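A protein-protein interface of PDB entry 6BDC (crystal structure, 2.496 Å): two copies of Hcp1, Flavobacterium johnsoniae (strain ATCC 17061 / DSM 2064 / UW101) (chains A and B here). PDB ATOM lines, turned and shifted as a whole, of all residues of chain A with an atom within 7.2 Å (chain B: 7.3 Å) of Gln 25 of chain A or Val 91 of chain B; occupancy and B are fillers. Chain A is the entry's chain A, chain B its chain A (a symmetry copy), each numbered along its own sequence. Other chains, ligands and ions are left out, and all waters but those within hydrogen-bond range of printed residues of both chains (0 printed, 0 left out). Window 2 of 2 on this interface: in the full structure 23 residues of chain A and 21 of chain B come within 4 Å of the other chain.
O of Leu 23 of chain A lies within hydrogen-bond range of N of Tyr 93 of chain B, at 2.9 Å.
NE2 of Gln 25 of chain A lies within hydrogen-bond range of O of Met 90 of chain B, at 2.8 Å.
The backbone NH of Gln 25 of chain A is in hydrogen-bond range of the backbone carbonyl oxygen of Val 91 of chain B (2.9 Å).
The backbone NH of Gly 31 of chain A sits close to the side-chain hydroxyl of Ser 112 of chain B (3.4 Å).
N of Arg 38 of chain A sits at hydrogen-bond distance from O of Ala 24 of chain A (3.0 Å).
The backbone NH (N) of Thr 35 of chain A lies within hydrogen-bond range of the backbone carbonyl oxygen (O) of Glu 26 of chain A.
N of Tyr 89 of chain B is in hydrogen-bond range of O of Ser 112 of chain B.
The backbone carbonyl oxygen (O) of Met 110 of chain B sits at hydrogen-bond distance from the backbone NH (N) of Val 91 of chain B.
The backbone NH (N) of Met 110 of chain B lies within hydrogen-bond range of the backbone carbonyl oxygen (O) of Lys 92 of chain B.
O of Leu 23 of chain A touches SD of Met 58 of chain B (3.8 Å).
Leu 23 of chain A touches Lys 92 of chain B (O to CA, 3.4 Å).
O of Val 91 of chain B touches CA of Ala 24 of chain A, at 3.3 Å.
Gln 25 of chain A touches Met 58 of chain B.
CA of Asn 61 of chain B touches NE2 of Gln 25 of chain A, 3.8 Å away.
Arg 41 of chain B touches Thr 27 of chain A (NE to OG1, 3.9 Å).
Val 91 of chain B touches Thr 27 of chain A.
Thr 35 of chain A touches Phe 62 of chain B.
Thr 37 of chain A touches Met 58 of chain B (CG2 to CE, 3.96 Å).
Gln 25 of chain A touches four residues of chain B.
Of the printed residues of chain B, Thr 27 of chain A touches Arg 41 and Val 91.
Arg 38 of chain A touches none of the printed residues of chain B.
Thr 59 of chain B touches none of the printed residues of chain A.
Val 91 of chain B touches three residues of chain A.
Printed residues of chain A within 4 Å of Ser 112 of chain B: Gly 31 (2.8 Å).
The nearest residue of chain A that does not touch Val 91 of chain B is Leu 23 of chain A (4.3 Å).
The nearest printed residue of chain A that does not touch Ser 112 of chain B is Arg 32 of chain A (4.9 Å).
Printed residues of chain A that touch a printed residue of chain B: Leu 23, Ala 24, Gln 25, Thr 27, Gly 31, Thr 35 and Thr 37.
Hydrophobic or aromatic side chains of chain A that line the printed part of chain B: Leu 23 and Ala 24.
Hydrophobic or aromatic side chains of chain B within 4 Å of the printed part of chain A: Met 58, Phe 62 and Val 91.
Among the printed residues, 13 pairs touch across the chains.
Among the printed residues, no Asp or Glu carboxylate lies within 4 Å of a Lys or Arg side-chain nitrogen of the other chain.
No position is printed for both chains.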
ATOM      1  N   LEU A  23      21.849 -21.824 -13.809  1.00  0.00           N
ATOM      2  CA  LEU A  23      21.966 -22.200 -12.411  1.00  0.00           C
ATOM      3  C   LEU A  23      20.679 -22.882 -11.977  1.00  0.00           C
ATOM      4  O   LEU A  23      19.594 -22.573 -12.479  1.00  0.00           O
ATOM      5  CB  LEU A  23      22.228 -20.991 -11.503  1.00  0.00           C
ATOM      6  CG  LEU A  23      23.345 -20.014 -11.869  1.00  0.00           C
ATOM      7  CD1 LEU A  23      22.848 -18.927 -12.809  1.00  0.00           C
ATOM      8  CD2 LEU A  23      23.928 -19.393 -10.613  1.00  0.00           C
ATOM      9  N   ALA A  24      20.802 -23.795 -11.019  1.00  0.00           N
ATOM     10  CA  ALA A  24      19.648 -24.569 -10.603  1.00  0.00           C
ATOM     11  C   ALA A  24      19.853 -25.108  -9.197  1.00  0.00           C
ATOM     12  O   ALA A  24      20.970 -25.448  -8.796  1.00  0.00           O
ATOM     13  CB  ALA A  24      19.379 -25.723 -11.576  1.00  0.00           C
ATOM     14  N   GLN A  25      18.755 -25.174  -8.454  1.00  0.00           N
ATOM     15  CA  GLN A  25      18.688 -25.897  -7.195  1.00  0.00           C
ATOM     16  C   GLN A  25      17.538 -26.893  -7.265  1.00  0.00           C
ATOM     17  O   GLN A  25      16.504 -26.627  -7.882  1.00  0.00           O
ATOM     18  CB  GLN A  25      18.509 -24.944  -6.000  1.00  0.00           C
ATOM     19  CG  GLN A  25      17.672 -23.707  -6.280  1.00  0.00           C
ATOM     20  CD  GLN A  25      17.305 -22.964  -5.006  1.00  0.00           C
ATOM     21  OE1 GLN A  25      17.222 -23.562  -3.934  1.00  0.00           O
ATOM     22  NE2 GLN A  25      17.089 -21.656  -5.116  1.00  0.00           N
ATOM     23  N   GLU A  26      17.731 -28.054  -6.648  1.00  0.00           N
ATOM     24  CA  GLU A  26      16.717 -29.098  -6.693  1.00  0.00           C
ATOM     25  C   GLU A  26      15.609 -28.815  -5.684  1.00  0.00           C
ATOM     26  O   GLU A  26      15.835 -28.191  -4.647  1.00  0.00           O
ATOM     27  CB  GLU A  26      17.336 -30.464  -6.401  1.00  0.00           C
ATOM     28  CG  GLU A  26      18.749 -30.629  -6.908  1.00  0.00           C
ATOM     29  CD  GLU A  26      19.560 -31.542  -6.017  1.00  0.00           C
ATOM     30  OE1 GLU A  26      19.874 -31.132  -4.878  1.00  0.00           O
ATOM     31  OE2 GLU A  26      19.865 -32.675  -6.444  1.00  0.00           O
ATOM     32  N   THR A  27      14.404 -29.286  -5.996  1.00  0.00           N
ATOM     33  CA  THR A  27      13.263 -29.168  -5.103  1.00  0.00           C
ATOM     34  C   THR A  27      12.835 -30.549  -4.626  1.00  0.00           C
ATOM     35  O   THR A  27      12.998 -31.545  -5.333  1.00  0.00           O
ATOM     36  CB  THR A  27      12.081 -28.476  -5.791  1.00  0.00           C
ATOM     37  OG1 THR A  27      11.634 -29.266  -6.902  1.00  0.00           O
ATOM     38  CG2 THR A  27      12.485 -27.100  -6.280  1.00  0.00           C
ATOM     39  N   GLY A  31       7.740 -27.870  -4.866  1.00  0.00           N
ATOM     40  CA  GLY A  31       8.455 -26.750  -4.285  1.00  0.00           C
ATOM     41  C   GLY A  31       9.454 -27.397  -3.371  1.00  0.00           C
ATOM     42  O   GLY A  31      10.137 -28.316  -3.793  1.00  0.00           O
ATOM     43  N   ARG A  32       9.510 -26.984  -2.114  1.00  0.00           N
ATOM     44  CA  ARG A  32      10.327 -27.709  -1.165  1.00  0.00           C
ATOM     45  C   ARG A  32      11.745 -27.781  -1.689  1.00  0.00           C
ATOM     46  O   ARG A  32      12.319 -28.867  -1.788  1.00  0.00           O
ATOM     47  CB  ARG A  32       9.761 -29.122  -0.966  1.00  0.00           C
ATOM     48  N   PRO A  33      12.345 -26.629  -1.928  1.00  0.00           N
ATOM     49  CA  PRO A  33      13.643 -26.625  -2.562  1.00  0.00           C
ATOM     50  C   PRO A  33      14.557 -27.474  -1.742  1.00  0.00           C
ATOM     51  O   PRO A  33      14.609 -27.308  -0.537  1.00  0.00           O
ATOM     52  CB  PRO A  33      14.054 -25.173  -2.426  1.00  0.00           C
ATOM     53  CG  PRO A  33      12.766 -24.417  -2.462  1.00  0.00           C
ATOM     54  CD  PRO A  33      11.643 -25.370  -2.184  1.00  0.00           C
ATOM     55  N   SER A  34      15.255 -28.389  -2.401  1.00  0.00           N
ATOM     56  CA  SER A  34      16.228 -29.247  -1.746  1.00  0.00           C
ATOM     57  C   SER A  34      17.337 -28.361  -1.242  1.00  0.00           C
ATOM     58  O   SER A  34      17.908 -28.580  -0.185  1.00  0.00           O
ATOM     59  CB  SER A  34      16.777 -30.286  -2.717  1.00  0.00           C
ATOM     60  N   THR A  35      17.659 -27.369  -2.051  1.00  0.00           N
ATOM     61  CA  THR A  35      18.677 -26.391  -1.731  1.00  0.00           C
ATOM     62  C   THR A  35      20.032 -26.962  -2.085  1.00  0.00           C
ATOM     63  O   THR A  35      20.145 -28.120  -2.450  1.00  0.00           O
ATOM     64  CB  THR A  35      18.625 -25.953  -0.269  1.00  0.00           C
ATOM     65  OG1 THR A  35      19.356 -26.882   0.532  1.00  0.00           O
ATOM     66  CG2 THR A  35      17.200 -25.903   0.204  1.00  0.00           C
ATOM     67  N   VAL A  36      21.038 -26.113  -2.023  1.00  0.00           N
ATOM     68  CA  VAL A  36      22.320 -26.408  -2.595  1.00  0.00           C
ATOM     69  C   VAL A  36      22.078 -25.877  -3.976  1.00  0.00           C
ATOM     70  O   VAL A  36      20.957 -25.907  -4.441  1.00  0.00           O
ATOM     71  CB  VAL A  36      22.559 -27.913  -2.678  1.00  0.00           C
ATOM     72  N   THR A  37      23.110 -25.417  -4.647  1.00  0.00           N
ATOM     73  CA  THR A  37      22.916 -24.791  -5.928  1.00  0.00           C
ATOM     74  C   THR A  37      24.087 -25.124  -6.808  1.00  0.00           C
ATOM     75  O   THR A  37      25.164 -25.405  -6.316  1.00  0.00           O
ATOM     76  CB  THR A  37      22.802 -23.281  -5.751  1.00  0.00           C
ATOM     77  OG1 THR A  37      22.154 -23.023  -4.512  1.00  0.00           O
ATOM     78  CG2 THR A  37      21.983 -22.686  -6.830  1.00  0.00           C
ATOM     79  N   ARG A  38      23.870 -25.108  -8.111  1.00  0.00           N
ATOM     80  CA  ARG A  38      24.936 -25.333  -9.051  1.00  0.00           C
ATOM     81  C   ARG A  38      24.991 -24.131  -9.938  1.00  0.00           C
ATOM     82  O   ARG A  38      23.975 -23.613 -10.338  1.00  0.00           O
ATOM     83  CB  ARG A  38      24.675 -26.582  -9.871  1.00  0.00           C
ATOM     84  N   ARG B  41       4.517 -24.984 -10.227  1.00  0.00           N
ATOM     85  CA  ARG B  41       5.705 -24.692 -11.018  1.00  0.00           C
ATOM     86  C   ARG B  41       5.306 -23.951 -12.287  1.00  0.00           C
ATOM     87  O   ARG B  41       4.392 -24.375 -13.001  1.00  0.00           O
ATOM     88  CB  ARG B  41       6.453 -25.978 -11.364  1.00  0.00           C
ATOM     89  CG  ARG B  41       7.499 -26.387 -10.334  1.00  0.00           C
ATOM     90  CD  ARG B  41       7.856 -27.862 -10.444  1.00  0.00           C
ATOM     91  NE  ARG B  41       8.913 -28.243  -9.509  1.00  0.00           N
ATOM     92  N   TRP B  57      17.786 -12.618  -8.425  1.00  0.00           N
ATOM     93  CA  TRP B  57      16.838 -13.463  -7.707  1.00  0.00           C
ATOM     94  C   TRP B  57      17.324 -14.904  -7.656  1.00  0.00           C
ATOM     95  O   TRP B  57      17.229 -15.564  -6.614  1.00  0.00           O
ATOM     96  CB  TRP B  57      15.460 -13.373  -8.370  1.00  0.00           C
ATOM     97  CG  TRP B  57      14.355 -14.131  -7.676  1.00  0.00           C
ATOM     98  CD1 TRP B  57      14.427 -14.811  -6.492  1.00  0.00           C
ATOM     99  CD2 TRP B  57      13.010 -14.279  -8.140  1.00  0.00           C
ATOM    100  NE1 TRP B  57      13.210 -15.375  -6.194  1.00  0.00           N
ATOM    101  CE2 TRP B  57      12.323 -15.061  -7.189  1.00  0.00           C
ATOM    102  CE3 TRP B  57      12.321 -13.827  -9.270  1.00  0.00           C
ATOM    103  CZ2 TRP B  57      10.980 -15.398  -7.336  1.00  0.00           C
ATOM    104  CZ3 TRP B  57      10.990 -14.161  -9.412  1.00  0.00           C
ATOM    105  CH2 TRP B  57      10.333 -14.941  -8.451  1.00  0.00           C
ATOM    106  N   MET B  58      17.857 -15.406  -8.765  1.00  0.00           N
ATOM    107  CA  MET B  58      18.401 -16.753  -8.788  1.00  0.00           C
ATOM    108  C   MET B  58      19.593 -16.889  -7.845  1.00  0.00           C
ATOM    109  O   MET B  58      19.739 -17.902  -7.165  1.00  0.00           O
ATOM    110  CB  MET B  58      18.817 -17.144 -10.206  1.00  0.00           C
ATOM    111  CG  MET B  58      19.414 -18.538 -10.303  1.00  0.00           C
ATOM    112  SD  MET B  58      18.083 -19.958 -10.114  1.00  0.00           S
ATOM    113  CE  MET B  58      18.932 -20.966  -8.673  1.00  0.00           C
ATOM    114  N   THR B  59      20.413 -15.860  -7.831  1.00  0.00           N
ATOM    115  CA  THR B  59      21.529 -15.756  -6.930  1.00  0.00           C
ATOM    116  C   THR B  59      21.062 -15.710  -5.499  1.00  0.00           C
ATOM    117  O   THR B  59      21.642 -16.344  -4.631  1.00  0.00           O
ATOM    118  CB  THR B  59      22.156 -14.417  -7.155  1.00  0.00           C
ATOM    119  OG1 THR B  59      21.095 -13.457  -7.126  1.00  0.00           O
ATOM    120  CG2 THR B  59      22.789 -14.391  -8.498  1.00  0.00           C
ATOM    121  N   ASN B  60      20.016 -14.934  -5.248  1.00  0.00           N
ATOM    122  CA  ASN B  60      19.508 -14.755  -3.894  1.00  0.00           C
ATOM    123  C   ASN B  60      19.023 -16.055  -3.293  1.00  0.00           C
ATOM    124  O   ASN B  60      19.209 -16.305  -2.113  1.00  0.00           O
ATOM    125  CB  ASN B  60      18.391 -13.720  -3.863  1.00  0.00           C
ATOM    126  N   ASN B  61      18.381 -16.877  -4.110  1.00  0.00           N
ATOM    127  CA  ASN B  61      18.022 -18.220  -3.684  1.00  0.00           C
ATOM    128  C   ASN B  61      16.740 -18.263  -2.900  1.00  0.00           C
ATOM    129  O   ASN B  61      15.665 -18.423  -3.461  1.00  0.00           O
ATOM    130  CB  ASN B  61      19.154 -18.889  -2.896  1.00  0.00           C
ATOM    131  N   PHE B  62      16.872 -18.158  -1.591  1.00  0.00           N
ATOM    132  CA  PHE B  62      15.772 -18.374  -0.683  1.00  0.00           C
ATOM    133  C   PHE B  62      14.701 -17.311  -0.804  1.00  0.00           C
ATOM    134  O   PHE B  62      13.630 -17.437  -0.254  1.00  0.00           O
ATOM    135  CB  PHE B  62      16.292 -18.444   0.731  1.00  0.00           C
ATOM    136  CG  PHE B  62      16.865 -19.776   1.090  1.00  0.00           C
ATOM    137  CD1 PHE B  62      16.139 -20.925   0.885  1.00  0.00           C
ATOM    138  CD2 PHE B  62      18.124 -19.875   1.639  1.00  0.00           C
ATOM    139  CE1 PHE B  62      16.657 -22.157   1.220  1.00  0.00           C
ATOM    140  CE2 PHE B  62      18.651 -21.101   1.976  1.00  0.00           C
ATOM    141  CZ  PHE B  62      17.917 -22.245   1.767  1.00  0.00           C
ATOM    142  N   GLU B  63      15.005 -16.228  -1.483  1.00  0.00           N
ATOM    143  CA  GLU B  63      14.011 -15.168  -1.584  1.00  0.00           C
ATOM    144  C   GLU B  63      12.760 -15.671  -2.289  1.00  0.00           C
ATOM    145  O   GLU B  63      12.832 -16.251  -3.377  1.00  0.00           O
ATOM    146  CB  GLU B  63      14.593 -13.969  -2.333  1.00  0.00           C
ATOM    147  CG  GLU B  63      13.599 -12.847  -2.619  1.00  0.00           C
ATOM    148  CD  GLU B  63      14.224 -11.674  -3.362  1.00  0.00           C
ATOM    149  OE1 GLU B  63      15.303 -11.849  -3.972  1.00  0.00           O
ATOM    150  OE2 GLU B  63      13.637 -10.572  -3.333  1.00  0.00           O
ATOM    151  N   ALA B  88       6.778 -17.529  -4.348  1.00  0.00           N
ATOM    152  CA  ALA B  88       7.462 -18.387  -5.310  1.00  0.00           C
ATOM    153  C   ALA B  88       8.972 -18.257  -5.170  1.00  0.00           C
ATOM    154  O   ALA B  88       9.500 -17.153  -5.023  1.00  0.00           O
ATOM    155  CB  ALA B  88       7.052 -18.041  -6.741  1.00  0.00           C
ATOM    156  N   TYR B  89       9.667 -19.388  -5.240  1.00  0.00           N
ATOM    157  CA  TYR B  89      11.116 -19.424  -5.092  1.00  0.00           C
ATOM    158  C   TYR B  89      11.777 -19.711  -6.433  1.00  0.00           C
ATOM    159  O   TYR B  89      11.305 -20.556  -7.201  1.00  0.00           O
ATOM    160  CB  TYR B  89      11.530 -20.478  -4.060  1.00  0.00           C
ATOM    161  N   MET B  90      12.866 -18.994  -6.716  1.00  0.00           N
ATOM    162  CA  MET B  90      13.652 -19.236  -7.922  1.00  0.00           C
ATOM    163  C   MET B  90      14.347 -20.593  -7.833  1.00  0.00           C
ATOM    164  O   MET B  90      15.116 -20.840  -6.908  1.00  0.00           O
ATOM    165  CB  MET B  90      14.682 -18.123  -8.133  1.00  0.00           C
ATOM    166  CG  MET B  90      14.348 -17.154  -9.258  1.00  0.00           C
ATOM    167  SD  MET B  90      14.711 -17.868 -11.028  1.00  0.00           S
ATOM    168  CE  MET B  90      14.610 -16.198 -12.037  1.00  0.00           C
ATOM    169  N   VAL B  91      14.071 -21.468  -8.800  1.00  0.00           N
ATOM    170  CA  VAL B  91      14.542 -22.844  -8.780  1.00  0.00           C
ATOM    171  C   VAL B  91      15.552 -23.114  -9.883  1.00  0.00           C
ATOM    172  O   VAL B  91      16.587 -23.746  -9.644  1.00  0.00           O
ATOM    173  CB  VAL B  91      13.356 -23.830  -8.873  1.00  0.00           C
ATOM    174  CG1 VAL B  91      13.857 -25.254  -9.051  1.00  0.00           C
ATOM    175  CG2 VAL B  91      12.502 -23.723  -7.622  1.00  0.00           C
ATOM    176  N   LYS B  92      15.273 -22.654 -11.099  1.00  0.00           N
ATOM    177  CA  LYS B  92      16.195 -22.806 -12.213  1.00  0.00           C
ATOM    178  C   LYS B  92      16.203 -21.519 -13.021  1.00  0.00           C
ATOM    179  O   LYS B  92      15.203 -20.797 -13.077  1.00  0.00           O
ATOM    180  CB  LYS B  92      15.826 -23.991 -13.115  1.00  0.00           C
ATOM    181  N   TYR B  93      17.340 -21.247 -13.659  1.00  0.00           N
ATOM    182  CA  TYR B  93      17.521 -20.030 -14.437  1.00  0.00           C
ATOM    183  C   TYR B  93      18.534 -20.302 -15.537  1.00  0.00           C
ATOM    184  O   TYR B  93      19.502 -21.035 -15.321  1.00  0.00           O
ATOM    185  CB  TYR B  93      17.993 -18.866 -13.556  1.00  0.00           C
ATOM    186  CG  TYR B  93      18.319 -17.592 -14.306  1.00  0.00           C
ATOM    187  CD1 TYR B  93      17.344 -16.628 -14.527  1.00  0.00           C
ATOM    188  CD2 TYR B  93      19.600 -17.350 -14.784  1.00  0.00           C
ATOM    189  CE1 TYR B  93      17.636 -15.456 -15.208  1.00  0.00           C
ATOM    190  CE2 TYR B  93      19.902 -16.182 -15.467  1.00  0.00           C
ATOM    191  CZ  TYR B  93      18.917 -15.239 -15.677  1.00  0.00           C
ATOM    192  OH  TYR B  93      19.210 -14.077 -16.358  1.00  0.00           O
ATOM    193  N   PHE B 109      13.454 -19.350 -17.132  1.00  0.00           N
ATOM    194  CA  PHE B 109      13.583 -19.712 -15.730  1.00  0.00           C
ATOM    195  C   PHE B 109      12.308 -20.393 -15.259  1.00  0.00           C
ATOM    196  O   PHE B 109      11.254 -20.296 -15.895  1.00  0.00           O
ATOM    197  CB  PHE B 109      13.890 -18.483 -14.859  1.00  0.00           C
ATOM    198  CG  PHE B 109      12.862 -17.390 -14.960  1.00  0.00           C
ATOM    199  CD1 PHE B 109      11.860 -17.268 -14.012  1.00  0.00           C
ATOM    200  CD2 PHE B 109      12.900 -16.482 -16.004  1.00  0.00           C
ATOM    201  CE1 PHE B 109      10.914 -16.259 -14.104  1.00  0.00           C
ATOM    202  CE2 PHE B 109      11.960 -15.473 -16.105  1.00  0.00           C
ATOM    203  CZ  PHE B 109      10.966 -15.361 -15.154  1.00  0.00           C
ATOM    204  N   MET B 110      12.421 -21.085 -14.130  1.00  0.00           N
ATOM    205  CA  MET B 110      11.280 -21.747 -13.519  1.00  0.00           C
ATOM    206  C   MET B 110      11.194 -21.431 -12.023  1.00  0.00           C
ATOM    207  O   MET B 110      12.169 -21.585 -11.278  1.00  0.00           O
ATOM    208  CB  MET B 110      11.350 -23.256 -13.759  1.00  0.00           C
ATOM    209  CG  MET B 110      10.931 -24.138 -12.581  1.00  0.00           C
ATOM    210  SD  MET B 110      10.504 -25.956 -13.154  1.00  0.00           S
ATOM    211  CE  MET B 110      11.222 -26.946 -11.621  1.00  0.00           C
ATOM    212  N   ILE B 111      10.018 -20.968 -11.596  1.00  0.00           N
ATOM    213  CA  ILE B 111       9.762 -20.631 -10.202  1.00  0.00           C
ATOM    214  C   ILE B 111       8.784 -21.641  -9.626  1.00  0.00           C
ATOM    215  O   ILE B 111       7.950 -22.211 -10.339  1.00  0.00           O
ATOM    216  CB  ILE B 111       9.221 -19.195 -10.036  1.00  0.00           C
ATOM    217  CG1 ILE B 111       7.971 -18.979 -10.890  1.00  0.00           C
ATOM    218  CG2 ILE B 111      10.297 -18.181 -10.382  1.00  0.00           C
ATOM    219  CD1 ILE B 111       7.369 -17.593 -10.746  1.00  0.00           C
ATOM    220  N   SER B 112       8.888 -21.858  -8.320  1.00  0.00           N
ATOM    221  CA  SER B 112       8.034 -22.799  -7.602  1.00  0.00           C
ATOM    222  C   SER B 112       7.234 -22.029  -6.560  1.00  0.00           C
ATOM    223  O   SER B 112       7.783 -21.597  -5.542  1.00  0.00           O
ATOM    224  CB  SER B 112       8.864 -23.902  -6.950  1.00  0.00           C
ATOM    225  OG  SER B 112       8.040 -24.731  -6.162  1.00  0.00           O
ATOM    226  N   ALA B 113       5.940 -21.861  -6.810  1.00  0.00           N
ATOM    227  CA  ALA B 113       5.090 -21.026  -5.973  1.00  0.00           C
ATOM    228  C   ALA B 113       4.409 -21.846  -4.886  1.00  0.00           C
ATOM    229  O   ALA B 113       4.054 -23.009  -5.096  1.00  0.00           O
ATOM    230  CB  ALA B 113       4.033 -20.309  -6.812  1.00  0.00           C
